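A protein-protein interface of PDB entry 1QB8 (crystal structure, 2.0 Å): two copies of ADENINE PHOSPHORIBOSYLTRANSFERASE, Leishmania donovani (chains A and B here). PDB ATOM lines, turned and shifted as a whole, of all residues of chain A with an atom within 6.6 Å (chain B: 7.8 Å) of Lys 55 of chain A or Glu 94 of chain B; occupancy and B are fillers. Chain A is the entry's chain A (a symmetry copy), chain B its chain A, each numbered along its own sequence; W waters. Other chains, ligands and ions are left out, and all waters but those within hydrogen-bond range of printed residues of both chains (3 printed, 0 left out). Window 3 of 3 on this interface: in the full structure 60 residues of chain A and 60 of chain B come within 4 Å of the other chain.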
ATOM      1  N   SER A  50      12.452  22.034  20.976  1.00  0.00           N
ATOM      2  CA  SER A  50      11.194  22.747  20.802  1.00  0.00           C
ATOM      3  C   SER A  50      10.110  22.032  21.605  1.00  0.00           C
ATOM      4  O   SER A  50       9.526  21.052  21.139  1.00  0.00           O
ATOM      5  CB  SER A  50      10.815  22.784  19.321  1.00  0.00           C
ATOM      6  OG  SER A  50       9.555  23.405  19.140  1.00  0.00           O
ATOM      7  N   PRO A  51       9.835  22.509  22.830  1.00  0.00           N
ATOM      8  CA  PRO A  51       8.822  21.909  23.701  1.00  0.00           C
ATOM      9  C   PRO A  51       7.460  21.744  23.036  1.00  0.00           C
ATOM     10  O   PRO A  51       6.847  20.679  23.125  1.00  0.00           O
ATOM     11  CB  PRO A  51       8.764  22.887  24.875  1.00  0.00           C
ATOM     12  CG  PRO A  51      10.164  23.371  24.966  1.00  0.00           C
ATOM     13  CD  PRO A  51      10.512  23.627  23.517  1.00  0.00           C
ATOM     14  N   GLU A  52       7.006  22.793  22.354  1.00  0.00           N
ATOM     15  CA  GLU A  52       5.713  22.773  21.672  1.00  0.00           C
ATOM     16  C   GLU A  52       5.685  21.693  20.584  1.00  0.00           C
ATOM     17  O   GLU A  52       4.720  20.938  20.476  1.00  0.00           O
ATOM     18  CB  GLU A  52       5.412  24.158  21.077  1.00  0.00           C
ATOM     19  CG  GLU A  52       3.974  24.347  20.590  1.00  0.00           C
ATOM     20  CD  GLU A  52       3.714  25.717  19.940  1.00  0.00           C
ATOM     21  OE1 GLU A  52       4.685  26.445  19.621  1.00  0.00           O
ATOM     22  OE2 GLU A  52       2.525  26.052  19.738  1.00  0.00           O
ATOM     23  N   THR A  53       6.762  21.594  19.811  1.00  0.00           N
ATOM     24  CA  THR A  53       6.845  20.599  18.745  1.00  0.00           C
ATOM     25  C   THR A  53       6.983  19.168  19.288  1.00  0.00           C
ATOM     26  O   THR A  53       6.349  18.243  18.780  1.00  0.00           O
ATOM     27  CB  THR A  53       8.012  20.892  17.772  1.00  0.00           C
ATOM     28  OG1 THR A  53       7.963  22.258  17.347  1.00  0.00           O
ATOM     29  CG2 THR A  53       7.904  20.016  16.549  1.00  0.00           C
ATOM     30  N   LEU A  54       7.794  18.987  20.326  1.00  0.00           N
ATOM     31  CA  LEU A  54       7.979  17.660  20.902  1.00  0.00           C
ATOM     32  C   LEU A  54       6.654  17.115  21.458  1.00  0.00           C
ATOM     33  O   LEU A  54       6.278  15.970  21.199  1.00  0.00           O
ATOM     34  CB  LEU A  54       9.044  17.708  21.995  1.00  0.00           C
ATOM     35  CG  LEU A  54       9.583  16.349  22.427  1.00  0.00           C
ATOM     36  CD1 LEU A  54      10.317  15.682  21.260  1.00  0.00           C
ATOM     37  CD2 LEU A  54      10.513  16.536  23.609  1.00  0.00           C
ATOM     38  N   LYS A  55       5.929  17.954  22.189  1.00  0.00           N
ATOM     39  CA  LYS A  55       4.640  17.563  22.761  1.00  0.00           C
ATOM     40  C   LYS A  55       3.589  17.264  21.684  1.00  0.00           C
ATOM     41  O   LYS A  55       2.762  16.368  21.850  1.00  0.00           O
ATOM     42  CB  LYS A  55       4.131  18.663  23.702  1.00  0.00           C
ATOM     43  CG  LYS A  55       2.833  18.341  24.416  1.00  0.00           C
ATOM     44  CD  LYS A  55       2.519  19.407  25.441  1.00  0.00           C
ATOM     45  CE  LYS A  55       1.202  19.125  26.130  1.00  0.00           C
ATOM     46  NZ  LYS A  55       0.939  20.127  27.203  1.00  0.00           N
ATOM     47  N   ALA A  56       3.615  18.024  20.588  1.00  0.00           N
ATOM     48  CA  ALA A  56       2.663  17.831  19.490  1.00  0.00           C
ATOM     49  C   ALA A  56       2.846  16.451  18.841  1.00  0.00           C
ATOM     50  O   ALA A  56       1.870  15.785  18.487  1.00  0.00           O
ATOM     51  CB  ALA A  56       2.819  18.939  18.458  1.00  0.00           C
ATOM     52  N   ILE A  57       4.103  16.031  18.705  1.00  0.00           N
ATOM     53  CA  ILE A  57       4.445  14.730  18.143  1.00  0.00           C
ATOM     54  C   ILE A  57       3.943  13.643  19.089  1.00  0.00           C
ATOM     55  O   ILE A  57       3.268  12.703  18.665  1.00  0.00           O
ATOM     56  CB  ILE A  57       5.977  14.584  17.968  1.00  0.00           C
ATOM     57  CG1 ILE A  57       6.478  15.565  16.904  1.00  0.00           C
ATOM     58  CG2 ILE A  57       6.349  13.143  17.638  1.00  0.00           C
ATOM     59  CD1 ILE A  57       7.987  15.639  16.771  1.00  0.00           C
ATOM     60  N   ARG A  58       4.248  13.804  20.375  1.00  0.00           N
ATOM     61  CA  ARG A  58       3.837  12.853  21.410  1.00  0.00           C
ATOM     62  C   ARG A  58       2.311  12.704  21.440  1.00  0.00           C
ATOM     63  O   ARG A  58       1.786  11.586  21.407  1.00  0.00           O
ATOM     64  CB  ARG A  58       4.356  13.328  22.782  1.00  0.00           C
ATOM     65  CG  ARG A  58       4.293  12.318  23.939  1.00  0.00           C
ATOM     66  CD  ARG A  58       2.893  12.157  24.562  1.00  0.00           C
ATOM     67  NE  ARG A  58       2.287  13.429  24.959  1.00  0.00           N
ATOM     68  CZ  ARG A  58       2.528  14.068  26.103  1.00  0.00           C
ATOM     69  NH1 ARG A  58       1.921  15.220  26.353  1.00  0.00           N
ATOM     70  NH2 ARG A  58       3.362  13.558  27.000  1.00  0.00           N
ATOM     71  N   ASP A  59       1.607  13.834  21.491  1.00  0.00           N
ATOM     72  CA  ASP A  59       0.144  13.839  21.541  1.00  0.00           C
ATOM     73  C   ASP A  59      -0.485  13.158  20.337  1.00  0.00           C
ATOM     74  O   ASP A  59      -1.356  12.303  20.490  1.00  0.00           O
ATOM     75  CB  ASP A  59      -0.398  15.277  21.653  1.00  0.00           C
ATOM     76  CG  ASP A  59      -0.096  15.925  23.002  1.00  0.00           C
ATOM     77  OD1 ASP A  59      -0.264  17.158  23.113  1.00  0.00           O
ATOM     78  OD2 ASP A  59       0.300  15.214  23.951  1.00  0.00           O
ATOM     79  N   PHE A  60      -0.004  13.518  19.149  1.00  0.00           N
ATOM     80  CA  PHE A  60      -0.517  12.965  17.905  1.00  0.00           C
ATOM     81  C   PHE A  60      -0.341  11.452  17.773  1.00  0.00           C
ATOM     82  O   PHE A  60      -1.307  10.733  17.505  1.00  0.00           O
ATOM     83  CB  PHE A  60       0.110  13.675  16.706  1.00  0.00           C
ATOM     84  CG  PHE A  60      -0.436  13.212  15.391  1.00  0.00           C
ATOM     85  CD1 PHE A  60      -1.613  13.754  14.887  1.00  0.00           C
ATOM     86  CD2 PHE A  60       0.203  12.206  14.674  1.00  0.00           C
ATOM     87  CE1 PHE A  60      -2.149  13.300  13.692  1.00  0.00           C
ATOM     88  CE2 PHE A  60      -0.326  11.741  13.476  1.00  0.00           C
ATOM     89  CZ  PHE A  60      -1.504  12.289  12.983  1.00  0.00           C
ATOM     90  N   MET A  88       8.523   8.215  24.936  1.00  0.00           N
ATOM     91  CA  MET A  88       7.437   9.082  25.391  1.00  0.00           C
ATOM     92  C   MET A  88       6.072   8.653  24.879  1.00  0.00           C
ATOM     93  O   MET A  88       5.039   9.007  25.450  1.00  0.00           O
ATOM     94  CB  MET A  88       7.714  10.557  25.088  1.00  0.00           C
ATOM     95  CG  MET A  88       7.816  10.929  23.633  1.00  0.00           C
ATOM     96  SD  MET A  88       8.259  12.673  23.481  1.00  0.00           S
ATOM     97  CE  MET A  88       7.990  12.888  21.716  1.00  0.00           C
ATOM     98  N   ARG B  66       9.133  19.742  38.873  1.00  0.00           N
ATOM     99  CA  ARG B  66       7.973  20.643  38.911  1.00  0.00           C
ATOM    100  C   ARG B  66       7.878  21.291  40.294  1.00  0.00           C
ATOM    101  O   ARG B  66       7.351  22.397  40.440  1.00  0.00           O
ATOM    102  CB  ARG B  66       6.670  19.892  38.613  1.00  0.00           C
ATOM    103  CG  ARG B  66       6.228  19.966  37.158  1.00  0.00           C
ATOM    104  CD  ARG B  66       4.871  19.307  36.949  1.00  0.00           C
ATOM    105  NE  ARG B  66       4.522  19.221  35.530  1.00  0.00           N
ATOM    106  CZ  ARG B  66       3.829  18.222  34.985  1.00  0.00           C
ATOM    107  NH1 ARG B  66       3.404  17.217  35.738  1.00  0.00           N
ATOM    108  NH2 ARG B  66       3.577  18.209  33.681  1.00  0.00           N
ATOM    109  N   PRO B  72      14.325  23.960  36.579  1.00  0.00           N
ATOM    110  CA  PRO B  72      15.321  23.731  35.528  1.00  0.00           C
ATOM    111  C   PRO B  72      14.819  24.347  34.225  1.00  0.00           C
ATOM    112  O   PRO B  72      13.619  24.477  34.016  1.00  0.00           O
ATOM    113  CB  PRO B  72      15.357  22.207  35.424  1.00  0.00           C
ATOM    114  CG  PRO B  72      15.023  21.767  36.815  1.00  0.00           C
ATOM    115  CD  PRO B  72      13.879  22.682  37.161  1.00  0.00           C
ATOM    116  N   THR B  73      15.737  24.740  33.360  1.00  0.00           N
ATOM    117  CA  THR B  73      15.360  25.338  32.093  1.00  0.00           C
ATOM    118  C   THR B  73      15.654  24.394  30.924  1.00  0.00           C
ATOM    119  O   THR B  73      15.077  24.538  29.846  1.00  0.00           O
ATOM    120  CB  THR B  73      16.121  26.656  31.867  1.00  0.00           C
ATOM    121  OG1 THR B  73      17.514  26.375  31.677  1.00  0.00           O
ATOM    122  CG2 THR B  73      15.958  27.581  33.074  1.00  0.00           C
ATOM    123  N   PRO B  87      13.748  13.114  27.068  1.00  0.00           N
ATOM    124  CA  PRO B  87      12.578  13.618  26.348  1.00  0.00           C
ATOM    125  C   PRO B  87      11.234  13.464  27.044  1.00  0.00           C
ATOM    126  O   PRO B  87      10.430  14.391  27.008  1.00  0.00           O
ATOM    127  CB  PRO B  87      12.631  12.846  25.034  1.00  0.00           C
ATOM    128  CG  PRO B  87      14.112  12.671  24.818  1.00  0.00           C
ATOM    129  CD  PRO B  87      14.572  12.260  26.191  1.00  0.00           C
ATOM    130  N   MET B  88      10.981  12.324  27.685  1.00  0.00           N
ATOM    131  CA  MET B  88       9.687  12.137  28.341  1.00  0.00           C
ATOM    132  C   MET B  88       9.508  13.008  29.574  1.00  0.00           C
ATOM    133  O   MET B  88       8.386  13.270  30.009  1.00  0.00           O
ATOM    134  CB  MET B  88       9.405  10.664  28.646  1.00  0.00           C
ATOM    135  CG  MET B  88      10.341   9.995  29.617  1.00  0.00           C
ATOM    136  SD  MET B  88       9.922   8.244  29.758  1.00  0.00           S
ATOM    137  CE  MET B  88      10.950   7.812  31.168  1.00  0.00           C
ATOM    138  N   ILE B  89      10.623  13.482  30.111  1.00  0.00           N
ATOM    139  CA  ILE B  89      10.586  14.361  31.266  1.00  0.00           C
ATOM    140  C   ILE B  89      10.435  15.779  30.744  1.00  0.00           C
ATOM    141  O   ILE B  89       9.582  16.531  31.212  1.00  0.00           O
ATOM    142  CB  ILE B  89      11.880  14.256  32.079  1.00  0.00           C
ATOM    143  CG1 ILE B  89      11.990  12.857  32.678  1.00  0.00           C
ATOM    144  CG2 ILE B  89      11.914  15.316  33.169  1.00  0.00           C
ATOM    145  CD1 ILE B  89      13.376  12.533  33.185  1.00  0.00           C
ATOM    146  N   ALA B  90      11.235  16.107  29.727  1.00  0.00           N
ATOM    147  CA  ALA B  90      11.227  17.434  29.111  1.00  0.00           C
ATOM    148  C   ALA B  90       9.896  17.801  28.471  1.00  0.00           C
ATOM    149  O   ALA B  90       9.458  18.944  28.577  1.00  0.00           O
ATOM    150  CB  ALA B  90      12.364  17.565  28.090  1.00  0.00           C
ATOM    151  N   VAL B  91       9.244  16.833  27.833  1.00  0.00           N
ATOM    152  CA  VAL B  91       7.952  17.075  27.187  1.00  0.00           C
ATOM    153  C   VAL B  91       6.889  17.468  28.221  1.00  0.00           C
ATOM    154  O   VAL B  91       5.999  18.268  27.935  1.00  0.00           O
ATOM    155  CB  VAL B  91       7.487  15.842  26.360  1.00  0.00           C
ATOM    156  CG1 VAL B  91       7.013  14.716  27.269  1.00  0.00           C
ATOM    157  CG2 VAL B  91       6.421  16.239  25.382  1.00  0.00           C
ATOM    158  N   GLU B  92       7.019  16.933  29.433  1.00  0.00           N
ATOM    159  CA  GLU B  92       6.091  17.239  30.515  1.00  0.00           C
ATOM    160  C   GLU B  92       6.396  18.585  31.168  1.00  0.00           C
ATOM    161  O   GLU B  92       5.484  19.340  31.503  1.00  0.00           O
ATOM    162  CB  GLU B  92       6.125  16.144  31.578  1.00  0.00           C
ATOM    163  CG  GLU B  92       5.675  14.787  31.085  1.00  0.00           C
ATOM    164  CD  GLU B  92       4.246  14.784  30.561  1.00  0.00           C
ATOM    165  OE1 GLU B  92       3.422  15.608  31.025  1.00  0.00           O
ATOM    166  OE2 GLU B  92       3.946  13.948  29.685  1.00  0.00           O
ATOM    167  N   LEU B  93       7.684  18.870  31.360  1.00  0.00           N
ATOM    168  CA  LEU B  93       8.127  20.120  31.974  1.00  0.00           C
ATOM    169  C   LEU B  93       8.082  21.274  30.985  1.00  0.00           C
ATOM    170  O   LEU B  93       8.229  22.432  31.369  1.00  0.00           O
ATOM    171  CB  LEU B  93       9.557  19.984  32.498  1.00  0.00           C
ATOM    172  CG  LEU B  93       9.870  18.926  33.557  1.00  0.00           C
ATOM    173  CD1 LEU B  93      11.353  18.960  33.844  1.00  0.00           C
ATOM    174  CD2 LEU B  93       9.087  19.183  34.819  1.00  0.00           C
ATOM    175  N   GLU B  94       7.923  20.945  29.705  1.00  0.00           N
ATOM    176  CA  GLU B  94       7.867  21.938  28.639  1.00  0.00           C
ATOM    177  C   GLU B  94       9.135  22.785  28.514  1.00  0.00           C
ATOM    178  O   GLU B  94       9.080  24.009  28.406  1.00  0.00           O
ATOM    179  CB  GLU B  94       6.619  22.814  28.793  1.00  0.00           C
ATOM    180  CG  GLU B  94       5.322  22.013  28.661  1.00  0.00           C
ATOM    181  CD  GLU B  94       4.056  22.838  28.864  1.00  0.00           C
ATOM    182  OE1 GLU B  94       2.955  22.242  28.795  1.00  0.00           O
ATOM    183  OE2 GLU B  94       4.153  24.068  29.097  1.00  0.00           O
ATOM    184  N   ILE B  95      10.282  22.110  28.553  1.00  0.00           N
ATOM    185  CA  ILE B  95      11.577  22.759  28.405  1.00  0.00           C
ATOM    186  C   ILE B  95      12.343  21.958  27.356  1.00  0.00           C
ATOM    187  O   ILE B  95      12.036  20.789  27.116  1.00  0.00           O
ATOM    188  CB  ILE B  95      12.372  22.811  29.733  1.00  0.00           C
ATOM    189  CG1 ILE B  95      12.529  21.409  30.323  1.00  0.00           C
ATOM    190  CG2 ILE B  95      11.698  23.763  30.708  1.00  0.00           C
ATOM    191  CD1 ILE B  95      13.269  21.399  31.644  1.00  0.00           C
ATOM    192  N   PRO B  96      13.344  22.574  26.712  1.00  0.00           N
ATOM    193  CA  PRO B  96      14.136  21.896  25.680  1.00  0.00           C
ATOM    194  C   PRO B  96      14.948  20.700  26.164  1.00  0.00           C
ATOM    195  O   PRO B  96      15.338  20.639  27.331  1.00  0.00           O
ATOM    196  CB  PRO B  96      15.084  22.994  25.195  1.00  0.00           C
ATOM    197  CG  PRO B  96      14.382  24.272  25.555  1.00  0.00           C
ATOM    198  CD  PRO B  96      13.808  23.959  26.899  1.00  0.00           C
ATOM    199  N   PHE B  97      15.155  19.734  25.266  1.00  0.00           N
ATOM    200  CA  PHE B  97      15.989  18.573  25.545  1.00  0.00           C
ATOM    201  C   PHE B  97      17.161  18.705  24.580  1.00  0.00           C
ATOM    202  O   PHE B  97      16.983  18.636  23.366  1.00  0.00           O
ATOM    203  CB  PHE B  97      15.280  17.245  25.284  1.00  0.00           C
ATOM    204  CG  PHE B  97      16.197  16.053  25.396  1.00  0.00           C
ATOM    205  CD1 PHE B  97      16.629  15.609  26.643  1.00  0.00           C
ATOM    206  CD2 PHE B  97      16.686  15.419  24.257  1.00  0.00           C
ATOM    207  CE1 PHE B  97      17.533  14.556  26.756  1.00  0.00           C
ATOM    208  CE2 PHE B  97      17.590  14.370  24.360  1.00  0.00           C
ATOM    209  CZ  PHE B  97      18.013  13.939  25.613  1.00  0.00           C
HETATM  210  O   HOH W   1       1.768  16.870  28.844  1.00  0.00           O
HETATM  211  O   HOH W   2       6.462  20.095  26.052  1.00  0.00           O
HETATM  212  O   HOH W   3       3.098  19.565  29.690  1.00  0.00           O
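The side-chain carboxylate of Glu 92 of chain B lies within salt-bridge range of the guanidinium group of Arg 58 of chain A (2.8 Å).
NZ of Lys 55 of chain A lies within salt-bridge range of OE1 of Glu 94 of chain B, 3.3 Å away.
The guanidinium group (NH2) of Arg 66 of chain B is in salt-bridge range of the side-chain carboxylate (OE1) of Glu 92 of chain B (3.7 Å).
O of Ala 90 of chain B sits at hydrogen-bond distance from N of Ile 95 of chain B, at 3.3 Å.
The side-chain carboxylate of Asp 59 of chain A lies within salt-bridge range of the guanidinium group of Arg 58 of chain A (2.9 Å).
Pro 51 of chain A touches Glu 94 of chain B (CB to C, 3.7 Å).
Pro 51 of chain A touches Ile 95 of chain B (CG to C, 3.5 Å).
CG of Pro 51 of chain A touches N of Pro 96 of chain B (3.7 Å).
Val 91 of chain B touches Lys 55 of chain A.
Val 91 of chain B touches Arg 58 of chain A.
Met 88 of chain B touches Met 88 of chain A.
Printed residues of chain B within 4 Å of Lys 55 of chain A: Val 91 (3.4 Å) and Glu 94 (3.3 Å).
Glu 94 of chain B touches two residues of chain A.
No residue of chain B comes within 4 Å of Ala 56 of chain A.
Of the printed residues of chain B, Pro 51 of chain A touches Glu 94 (3.7 Å), Ile 95 (3.5 Å) and Pro 96 (3.7 Å).
Of the printed residues of chain A, Glu 92 of chain B touches Arg 58.
Printed residues of chain B within 4 Å of Met 88 of chain A: Met 88.
Of the printed residues of chain A, Met 88 of chain B touches Met 88.
Printed residues of chain A within 4 Å of Pro 96 of chain B: Pro 51 (3.7 Å).
Ala 90 of chain B touches none of the printed residues of chain A.
The nearest residue of chain A that does not touch Glu 94 of chain B is Glu 52 of chain A (6.4 Å).
Hydrophobic or aromatic side chains of chain B that line the printed part of chain A: Met 88 and Val 91.
Along chain B the printed residues that touch a printed residue of chain A span positions 88 to 96.
Of the 12 printed residues of chain A, 4 touch a printed residue of chain B.
Hydrophobic or aromatic side chains of chain A that line the printed part of chain B: Pro 51 and Met 88.
Among the printed residues, 8 pairs touch across the chains.
Among the printed residues, Asp or Glu carboxylates within 4 Å of a Lys or Arg side-chain nitrogen of the other chain: Lys 55 of chain A with Glu 94 of chain B (3.3 Å) and Arg 58 of chain A with Glu 92 of chain B (2.8 Å).
Met 88 of chain A touches its own counterpart, Met 88 of chain B.
Position printed for both chains: 88.
Water W2 bridges O of Val 91 of chain B (2.7 Å) and O of Pro 51 of chain A (3.0 Å).
Water W3 lies within hydrogen-bond range of OE1 of Glu 94 of chain B (2.8 Å), O of Glu 92 of chain B (3.0 Å) and NZ of Lys 55 of chain A (3.3 Å).
Water W1 bridges the guanidinium group of Arg 58 of chain A and the side-chain carboxylate of Glu 92 of chain B.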
